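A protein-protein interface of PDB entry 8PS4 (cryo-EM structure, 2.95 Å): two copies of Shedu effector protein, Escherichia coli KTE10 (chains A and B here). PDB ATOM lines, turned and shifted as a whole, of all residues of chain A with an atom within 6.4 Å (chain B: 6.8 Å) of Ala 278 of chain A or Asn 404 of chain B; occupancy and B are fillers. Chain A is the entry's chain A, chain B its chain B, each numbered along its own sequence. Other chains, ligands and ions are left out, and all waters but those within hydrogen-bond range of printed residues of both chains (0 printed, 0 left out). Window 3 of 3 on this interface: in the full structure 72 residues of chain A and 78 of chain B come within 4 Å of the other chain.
ND2 of Asn 404 of chain B lies within hydrogen-bond range of O of Ala 278 of chain A (3.0 Å). The side-chain amide nitrogen of Asn 404 of chain B sits close to the side-chain sulfur of Met 348 of chain A (3.8 Å). NH1 of Arg 401 of chain B sits at hydrogen-bond distance from OD1 of Asn 279 of chain A (3.1 Å).
The guanidinium group (NH2) of Arg 351 of chain A is in hydrogen-bond range of the backbone carbonyl oxygen (O) of Asn 279 of chain A (2.5 Å). The backbone carbonyl oxygen (O) of Val 276 of chain A sits at hydrogen-bond distance from the backbone NH (N) of Ile 248 of chain A (2.8 Å). OD2 of Asp 277 of chain A lies close to OD1 of Asn 279 of chain A. The side-chain amide nitrogen (ND2) of Asn 404 of chain B sits close to the backbone carbonyl oxygen (O) of Arg 400 of chain B (3.3 Å). The backbone NH (N) of Ala 278 of chain A sits at hydrogen-bond distance from the backbone carbonyl oxygen (O) of Lys 246 of chain A (3.4 Å). The side-chain hydroxyl (OG1) of Thr 405 of chain B is in hydrogen-bond range of the backbone carbonyl oxygen (O) of Arg 401 of chain B, at 2.9 Å.
Among the printed residues, merely in contact across the chains: Ile 248 of chain A with Asn 404 of chain B (3.7 Å), Ile 248 of chain A with Thr 405 of chain B (3.6 Å), Ile 248 of chain A with Ala 408 of chain B (3.6 Å), Ala 278 of chain A with Arg 401 of chain B (3.96 Å), Pro 345 of chain A with Asn 404 of chain B (3.8 Å) and Pro 345 of chain A with Glu 407 of chain B (3.8 Å).
Printed residues of chain B within 4 Å of Ile 248 of chain A: Asn 404 (3.7 Å), Thr 405 (3.6 Å) and Ala 408 (3.6 Å). Printed residues of chain B within 4 Å of Met 348 of chain A: Asn 404 (3.7 Å). Arg 351 of chain A touches none of the printed residues of chain B. Asn 404 of chain B touches just these residues of chain A: Ile 248, Ala 278, Pro 345 and Met 348. Printed residues of chain A within 4 Å of Ala 408 of chain B: Ile 248.
Printed residues of chain A that touch a printed residue of chain B: Ile 248, Ala 278, Asn 279, Pro 345 and Met 348. Of the 12 printed residues of chain B, 5 touch a printed residue of chain A. Among the printed residues, no Asp or Glu carboxylate lies within 4 Å of a Lys or Arg side-chain nitrogen of the other chain.
No position is printed for both chains. Of the 9 pairs that touch across the chains among the printed residues, none has its exchanged pair printed and touching as well.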
ATOM      1  N   PRO A 245      18.757  12.207 -28.340  1.00  0.00           N
ATOM      2  CA  PRO A 245      19.688  13.329 -28.534  1.00  0.00           C
ATOM      3  C   PRO A 245      21.010  13.137 -27.778  1.00  0.00           C
ATOM      4  O   PRO A 245      21.997  13.723 -28.183  1.00  0.00           O
ATOM      5  CB  PRO A 245      18.918  14.534 -27.977  1.00  0.00           C
ATOM      6  CG  PRO A 245      17.475  14.108 -28.083  1.00  0.00           C
ATOM      7  CD  PRO A 245      17.514  12.644 -27.703  1.00  0.00           C
ATOM      8  N   LYS A 246      20.997  12.327 -26.716  1.00  0.00           N
ATOM      9  CA  LYS A 246      22.228  12.069 -25.925  1.00  0.00           C
ATOM     10  C   LYS A 246      23.274  11.481 -26.874  1.00  0.00           C
ATOM     11  O   LYS A 246      24.442  11.912 -26.801  1.00  0.00           O
ATOM     12  CB  LYS A 246      21.897  11.076 -24.806  1.00  0.00           C
ATOM     13  CG  LYS A 246      23.088  10.391 -24.152  1.00  0.00           C
ATOM     14  CD  LYS A 246      22.706   9.184 -23.324  1.00  0.00           C
ATOM     15  CE  LYS A 246      23.903   8.449 -22.762  1.00  0.00           C
ATOM     16  NZ  LYS A 246      23.506   7.198 -22.074  1.00  0.00           N
ATOM     17  N   TYR A 247      22.864  10.569 -27.757  1.00  0.00           N
ATOM     18  CA  TYR A 247      23.803  10.029 -28.775  1.00  0.00           C
ATOM     19  C   TYR A 247      23.879  11.041 -29.921  1.00  0.00           C
ATOM     20  O   TYR A 247      22.856  11.238 -30.607  1.00  0.00           O
ATOM     21  CB  TYR A 247      23.377   8.615 -29.171  1.00  0.00           C
ATOM     22  CG  TYR A 247      23.113   7.737 -27.975  1.00  0.00           C
ATOM     23  CD1 TYR A 247      24.151   7.299 -27.170  1.00  0.00           C
ATOM     24  CD2 TYR A 247      21.824   7.370 -27.627  1.00  0.00           C
ATOM     25  CE1 TYR A 247      23.917   6.504 -26.060  1.00  0.00           C
ATOM     26  CE2 TYR A 247      21.572   6.574 -26.523  1.00  0.00           C
ATOM     27  CZ  TYR A 247      22.623   6.138 -25.736  1.00  0.00           C
ATOM     28  OH  TYR A 247      22.382   5.355 -24.645  1.00  0.00           O
ATOM     29  N   ILE A 248      25.044  11.662 -30.120  1.00  0.00           N
ATOM     30  CA  ILE A 248      25.160  12.757 -31.130  1.00  0.00           C
ATOM     31  C   ILE A 248      25.473  12.176 -32.514  1.00  0.00           C
ATOM     32  O   ILE A 248      25.003  12.759 -33.510  1.00  0.00           O
ATOM     33  CB  ILE A 248      26.202  13.796 -30.671  1.00  0.00           C
ATOM     34  CG1 ILE A 248      27.612  13.207 -30.605  1.00  0.00           C
ATOM     35  CG2 ILE A 248      25.791  14.402 -29.340  1.00  0.00           C
ATOM     36  CD1 ILE A 248      28.676  14.216 -30.261  1.00  0.00           C
ATOM     37  N   VAL A 276      27.315   7.156 -30.595  1.00  0.00           N
ATOM     38  CA  VAL A 276      28.407   7.859 -29.857  1.00  0.00           C
ATOM     39  C   VAL A 276      27.796   8.957 -28.983  1.00  0.00           C
ATOM     40  O   VAL A 276      27.088   9.820 -29.533  1.00  0.00           O
ATOM     41  CB  VAL A 276      29.470   8.433 -30.812  1.00  0.00           C
ATOM     42  CG1 VAL A 276      30.705   8.896 -30.053  1.00  0.00           C
ATOM     43  CG2 VAL A 276      29.855   7.430 -31.887  1.00  0.00           C
ATOM     44  N   ASP A 277      28.077   8.929 -27.678  1.00  0.00           N
ATOM     45  CA  ASP A 277      27.557   9.947 -26.725  1.00  0.00           C
ATOM     46  C   ASP A 277      28.345  11.250 -26.900  1.00  0.00           C
ATOM     47  O   ASP A 277      29.427  11.201 -27.513  1.00  0.00           O
ATOM     48  CB  ASP A 277      27.651   9.409 -25.292  1.00  0.00           C
ATOM     49  CG  ASP A 277      27.033  10.292 -24.221  1.00  0.00           C
ATOM     50  OD1 ASP A 277      26.194  11.143 -24.568  1.00  0.00           O
ATOM     51  OD2 ASP A 277      27.401  10.120 -23.043  1.00  0.00           O
ATOM     52  N   ALA A 278      27.817  12.372 -26.402  1.00  0.00           N
ATOM     53  CA  ALA A 278      28.563  13.654 -26.438  1.00  0.00           C
ATOM     54  C   ALA A 278      29.847  13.475 -25.625  1.00  0.00           C
ATOM     55  O   ALA A 278      30.872  14.069 -26.005  1.00  0.00           O
ATOM     56  CB  ALA A 278      27.703  14.762 -25.887  1.00  0.00           C
ATOM     57  N   ASN A 279      29.784  12.709 -24.530  1.00  0.00           N
ATOM     58  CA  ASN A 279      30.993  12.403 -23.715  1.00  0.00           C
ATOM     59  C   ASN A 279      31.979  11.584 -24.555  1.00  0.00           C
ATOM     60  O   ASN A 279      33.182  11.612 -24.233  1.00  0.00           O
ATOM     61  CB  ASN A 279      30.629  11.663 -22.425  1.00  0.00           C
ATOM     62  CG  ASN A 279      29.839  12.517 -21.458  1.00  0.00           C
ATOM     63  OD1 ASN A 279      28.988  12.012 -20.729  1.00  0.00           O
ATOM     64  ND2 ASN A 279      30.110  13.811 -21.445  1.00  0.00           N
ATOM     65  N   GLY A 280      31.491  10.883 -25.583  1.00  0.00           N
ATOM     66  CA  GLY A 280      32.355  10.010 -26.404  1.00  0.00           C
ATOM     67  C   GLY A 280      32.194   8.553 -26.012  1.00  0.00           C
ATOM     68  O   GLY A 280      32.850   7.702 -26.640  1.00  0.00           O
ATOM     69  N   ASN A 281      31.308   8.274 -25.051  1.00  0.00           N
ATOM     70  CA  ASN A 281      31.026   6.871 -24.644  1.00  0.00           C
ATOM     71  C   ASN A 281      30.375   6.140 -25.824  1.00  0.00           C
ATOM     72  O   ASN A 281      29.697   6.806 -26.628  1.00  0.00           O
ATOM     73  CB  ASN A 281      30.139   6.819 -23.399  1.00  0.00           C
ATOM     74  CG  ASN A 281      30.706   7.610 -22.238  1.00  0.00           C
ATOM     75  OD1 ASN A 281      31.862   8.028 -22.268  1.00  0.00           O
ATOM     76  ND2 ASN A 281      29.902   7.817 -21.208  1.00  0.00           N
ATOM     77  N   PRO A 345      33.085  14.803 -33.843  1.00  0.00           N
ATOM     78  CA  PRO A 345      33.424  16.228 -33.784  1.00  0.00           C
ATOM     79  C   PRO A 345      34.878  16.365 -33.310  1.00  0.00           C
ATOM     80  O   PRO A 345      35.323  15.521 -32.558  1.00  0.00           O
ATOM     81  CB  PRO A 345      32.482  16.784 -32.706  1.00  0.00           C
ATOM     82  CG  PRO A 345      31.339  15.795 -32.667  1.00  0.00           C
ATOM     83  CD  PRO A 345      31.984  14.455 -32.943  1.00  0.00           C
ATOM     84  N   ALA A 346      35.580  17.410 -33.756  1.00  0.00           N
ATOM     85  CA  ALA A 346      37.014  17.555 -33.410  1.00  0.00           C
ATOM     86  C   ALA A 346      37.177  17.664 -31.891  1.00  0.00           C
ATOM     87  O   ALA A 346      36.338  18.330 -31.251  1.00  0.00           O
ATOM     88  CB  ALA A 346      37.593  18.757 -34.114  1.00  0.00           C
ATOM     89  N   GLY A 347      38.223  17.038 -31.341  1.00  0.00           N
ATOM     90  CA  GLY A 347      38.443  17.052 -29.880  1.00  0.00           C
ATOM     91  C   GLY A 347      37.655  15.964 -29.168  1.00  0.00           C
ATOM     92  O   GLY A 347      37.638  15.974 -27.921  1.00  0.00           O
ATOM     93  N   MET A 348      37.025  15.060 -29.925  1.00  0.00           N
ATOM     94  CA  MET A 348      36.245  13.946 -29.318  1.00  0.00           C
ATOM     95  C   MET A 348      36.860  12.598 -29.705  1.00  0.00           C
ATOM     96  O   MET A 348      37.153  12.407 -30.902  1.00  0.00           O
ATOM     97  CB  MET A 348      34.781  13.976 -29.764  1.00  0.00           C
ATOM     98  CG  MET A 348      33.864  14.636 -28.759  1.00  0.00           C
ATOM     99  SD  MET A 348      32.133  14.267 -29.119  1.00  0.00           S
ATOM    100  CE  MET A 348      32.209  12.483 -29.278  1.00  0.00           C
ATOM    101  N   ARG A 351      35.276   6.372 -26.408  1.00  0.00           N
ATOM    102  CA  ARG A 351      35.728   5.659 -25.183  1.00  0.00           C
ATOM    103  C   ARG A 351      34.734   4.526 -24.915  1.00  0.00           C
ATOM    104  O   ARG A 351      33.525   4.799 -24.971  1.00  0.00           O
ATOM    105  CB  ARG A 351      35.768   6.616 -23.989  1.00  0.00           C
ATOM    106  CG  ARG A 351      36.855   7.678 -24.068  1.00  0.00           C
ATOM    107  CD  ARG A 351      37.053   8.384 -22.742  1.00  0.00           C
ATOM    108  NE  ARG A 351      35.864   9.112 -22.322  1.00  0.00           N
ATOM    109  CZ  ARG A 351      35.573  10.353 -22.694  1.00  0.00           C
ATOM    110  NH1 ARG A 351      36.388  11.009 -23.502  1.00  0.00           N
ATOM    111  NH2 ARG A 351      34.468  10.932 -22.260  1.00  0.00           N
ATOM    112  N   ASP B 397      31.278  21.449 -18.278  1.00  0.00           N
ATOM    113  CA  ASP B 397      31.100  20.142 -18.968  1.00  0.00           C
ATOM    114  C   ASP B 397      29.802  20.178 -19.782  1.00  0.00           C
ATOM    115  O   ASP B 397      29.809  19.680 -20.924  1.00  0.00           O
ATOM    116  CB  ASP B 397      31.100  18.984 -17.967  1.00  0.00           C
ATOM    117  CG  ASP B 397      31.292  17.616 -18.598  1.00  0.00           C
ATOM    118  OD1 ASP B 397      31.705  17.563 -19.775  1.00  0.00           O
ATOM    119  OD2 ASP B 397      31.029  16.613 -17.907  1.00  0.00           O
ATOM    120  N   LEU B 399      28.313  22.759 -21.131  1.00  0.00           N
ATOM    121  CA  LEU B 399      28.521  23.621 -22.326  1.00  0.00           C
ATOM    122  C   LEU B 399      29.278  22.832 -23.399  1.00  0.00           C
ATOM    123  O   LEU B 399      28.917  22.953 -24.584  1.00  0.00           O
ATOM    124  CB  LEU B 399      29.306  24.869 -21.914  1.00  0.00           C
ATOM    125  CG  LEU B 399      28.592  25.808 -20.945  1.00  0.00           C
ATOM    126  CD1 LEU B 399      29.554  26.849 -20.398  1.00  0.00           C
ATOM    127  CD2 LEU B 399      27.401  26.476 -21.610  1.00  0.00           C
ATOM    128  N   ARG B 400      30.289  22.056 -22.990  1.00  0.00           N
ATOM    129  CA  ARG B 400      31.084  21.252 -23.957  1.00  0.00           C
ATOM    130  C   ARG B 400      30.179  20.212 -24.628  1.00  0.00           C
ATOM    131  O   ARG B 400      30.316  20.017 -25.847  1.00  0.00           O
ATOM    132  CB  ARG B 400      32.277  20.589 -23.262  1.00  0.00           C
ATOM    133  CG  ARG B 400      33.312  21.575 -22.741  1.00  0.00           C
ATOM    134  CD  ARG B 400      34.626  20.904 -22.386  1.00  0.00           C
ATOM    135  NE  ARG B 400      34.479  19.839 -21.407  1.00  0.00           N
ATOM    136  CZ  ARG B 400      34.629  19.992 -20.096  1.00  0.00           C
ATOM    137  NH1 ARG B 400      34.934  21.179 -19.599  1.00  0.00           N
ATOM    138  NH2 ARG B 400      34.478  18.958 -19.290  1.00  0.00           N
ATOM    139  N   ARG B 401      29.291  19.579 -23.856  1.00  0.00           N
ATOM    140  CA  ARG B 401      28.355  18.570 -24.422  1.00  0.00           C
ATOM    141  C   ARG B 401      27.430  19.245 -25.437  1.00  0.00           C
ATOM    142  O   ARG B 401      27.180  18.641 -26.498  1.00  0.00           O
ATOM    143  CB  ARG B 401      27.546  17.909 -23.304  1.00  0.00           C
ATOM    144  CG  ARG B 401      28.342  16.915 -22.471  1.00  0.00           C
ATOM    145  CD  ARG B 401      27.653  16.634 -21.152  1.00  0.00           C
ATOM    146  NE  ARG B 401      26.253  16.261 -21.302  1.00  0.00           N
ATOM    147  CZ  ARG B 401      25.804  15.012 -21.364  1.00  0.00           C
ATOM    148  NH1 ARG B 401      26.649  13.998 -21.286  1.00  0.00           N
ATOM    149  NH2 ARG B 401      24.511  14.782 -21.500  1.00  0.00           N
ATOM    150  N   LEU B 402      26.952  20.454 -25.125  1.00  0.00           N
ATOM    151  CA  LEU B 402      26.074  21.200 -26.065  1.00  0.00           C
ATOM    152  C   LEU B 402      26.857  21.493 -27.347  1.00  0.00           C
ATOM    153  O   LEU B 402      26.288  21.303 -28.436  1.00  0.00           O
ATOM    154  CB  LEU B 402      25.616  22.497 -25.391  1.00  0.00           C
ATOM    155  CG  LEU B 402      24.476  22.346 -24.385  1.00  0.00           C
ATOM    156  CD1 LEU B 402      24.539  23.428 -23.318  1.00  0.00           C
ATOM    157  CD2 LEU B 402      23.129  22.364 -25.089  1.00  0.00           C
ATOM    158  N   ASN B 403      28.126  21.893 -27.215  1.00  0.00           N
ATOM    159  CA  ASN B 403      28.972  22.196 -28.400  1.00  0.00           C
ATOM    160  C   ASN B 403      29.143  20.926 -29.240  1.00  0.00           C
ATOM    161  O   ASN B 403      29.054  21.027 -30.477  1.00  0.00           O
ATOM    162  CB  ASN B 403      30.332  22.769 -27.996  1.00  0.00           C
ATOM    163  CG  ASN B 403      30.279  24.248 -27.678  1.00  0.00           C
ATOM    164  OD1 ASN B 403      30.745  24.680 -26.627  1.00  0.00           O
ATOM    165  ND2 ASN B 403      29.708  25.029 -28.581  1.00  0.00           N
ATOM    166  N   ASN B 404      29.359  19.780 -28.588  1.00  0.00           N
ATOM    167  CA  ASN B 404      29.564  18.501 -29.319  1.00  0.00           C
ATOM    168  C   ASN B 404      28.296  18.167 -30.110  1.00  0.00           C
ATOM    169  O   ASN B 404      28.423  17.746 -31.275  1.00  0.00           O
ATOM    170  CB  ASN B 404      29.932  17.361 -28.368  1.00  0.00           C
ATOM    171  CG  ASN B 404      31.259  17.579 -27.672  1.00  0.00           C
ATOM    172  OD1 ASN B 404      32.112  18.313 -28.166  1.00  0.00           O
ATOM    173  ND2 ASN B 404      31.442  16.945 -26.526  1.00  0.00           N
ATOM    174  N   THR B 405      27.124  18.368 -29.500  1.00  0.00           N
ATOM    175  CA  THR B 405      25.840  18.068 -30.186  1.00  0.00           C
ATOM    176  C   THR B 405      25.702  18.975 -31.411  1.00  0.00           C
ATOM    177  O   THR B 405      25.327  18.462 -32.482  1.00  0.00           O
ATOM    178  CB  THR B 405      24.653  18.252 -29.230  1.00  0.00           C
ATOM    179  OG1 THR B 405      24.976  17.619 -27.992  1.00  0.00           O
ATOM    180  CG2 THR B 405      23.361  17.685 -29.776  1.00  0.00           C
ATOM    181  N   ILE B 406      26.036  20.260 -31.262  1.00  0.00           N
ATOM    182  CA  ILE B 406      25.902  21.229 -32.388  1.00  0.00           C
ATOM    183  C   ILE B 406      26.837  20.800 -33.524  1.00  0.00           C
ATOM    184  O   ILE B 406      26.384  20.789 -34.684  1.00  0.00           O
ATOM    185  CB  ILE B 406      26.216  22.656 -31.893  1.00  0.00           C
ATOM    186  CG1 ILE B 406      25.194  23.131 -30.860  1.00  0.00           C
ATOM    187  CG2 ILE B 406      26.328  23.630 -33.055  1.00  0.00           C
ATOM    188  CD1 ILE B 406      25.684  24.267 -29.992  1.00  0.00           C
ATOM    189  N   GLU B 407      28.075  20.419 -33.194  1.00  0.00           N
ATOM    190  CA  GLU B 407      29.064  20.034 -34.237  1.00  0.00           C
ATOM    191  C   GLU B 407      28.590  18.776 -34.973  1.00  0.00           C
ATOM    192  O   GLU B 407      28.737  18.728 -36.207  1.00  0.00           O
ATOM    193  CB  GLU B 407      30.454  19.843 -33.625  1.00  0.00           C
ATOM    194  CG  GLU B 407      31.049  21.127 -33.077  1.00  0.00           C
ATOM    195  CD  GLU B 407      31.197  22.249 -34.092  1.00  0.00           C
ATOM    196  OE1 GLU B 407      31.600  21.963 -35.237  1.00  0.00           O
ATOM    197  OE2 GLU B 407      30.901  23.407 -33.734  1.00  0.00           O
ATOM    198  N   ALA B 408      28.050  17.799 -34.237  1.00  0.00           N
ATOM    199  CA  ALA B 408      27.570  16.545 -34.863  1.00  0.00           C
ATOM    200  C   ALA B 408      26.409  16.853 -35.813  1.00  0.00           C
ATOM    201  O   ALA B 408      26.373  16.263 -36.910  1.00  0.00           O
ATOM    202  CB  ALA B 408      27.164  15.561 -33.799  1.00  0.00           C
ATOM    203  N   LEU B 409      25.497  17.739 -35.402  1.00  0.00           N
ATOM    204  CA  LEU B 409      24.353  18.131 -36.269  1.00  0.00           C
ATOM    205  C   LEU B 409      24.882  18.839 -37.522  1.00  0.00           C
ATOM    206  O   LEU B 409      24.341  18.581 -38.614  1.00  0.00           O
ATOM    207  CB  LEU B 409      23.410  19.034 -35.472  1.00  0.00           C
ATOM    208  CG  LEU B 409      22.577  18.335 -34.400  1.00  0.00           C
ATOM    209  CD1 LEU B 409      21.980  19.345 -33.434  1.00  0.00           C
ATOM    210  CD2 LEU B 409      21.484  17.485 -35.031  1.00  0.00           C
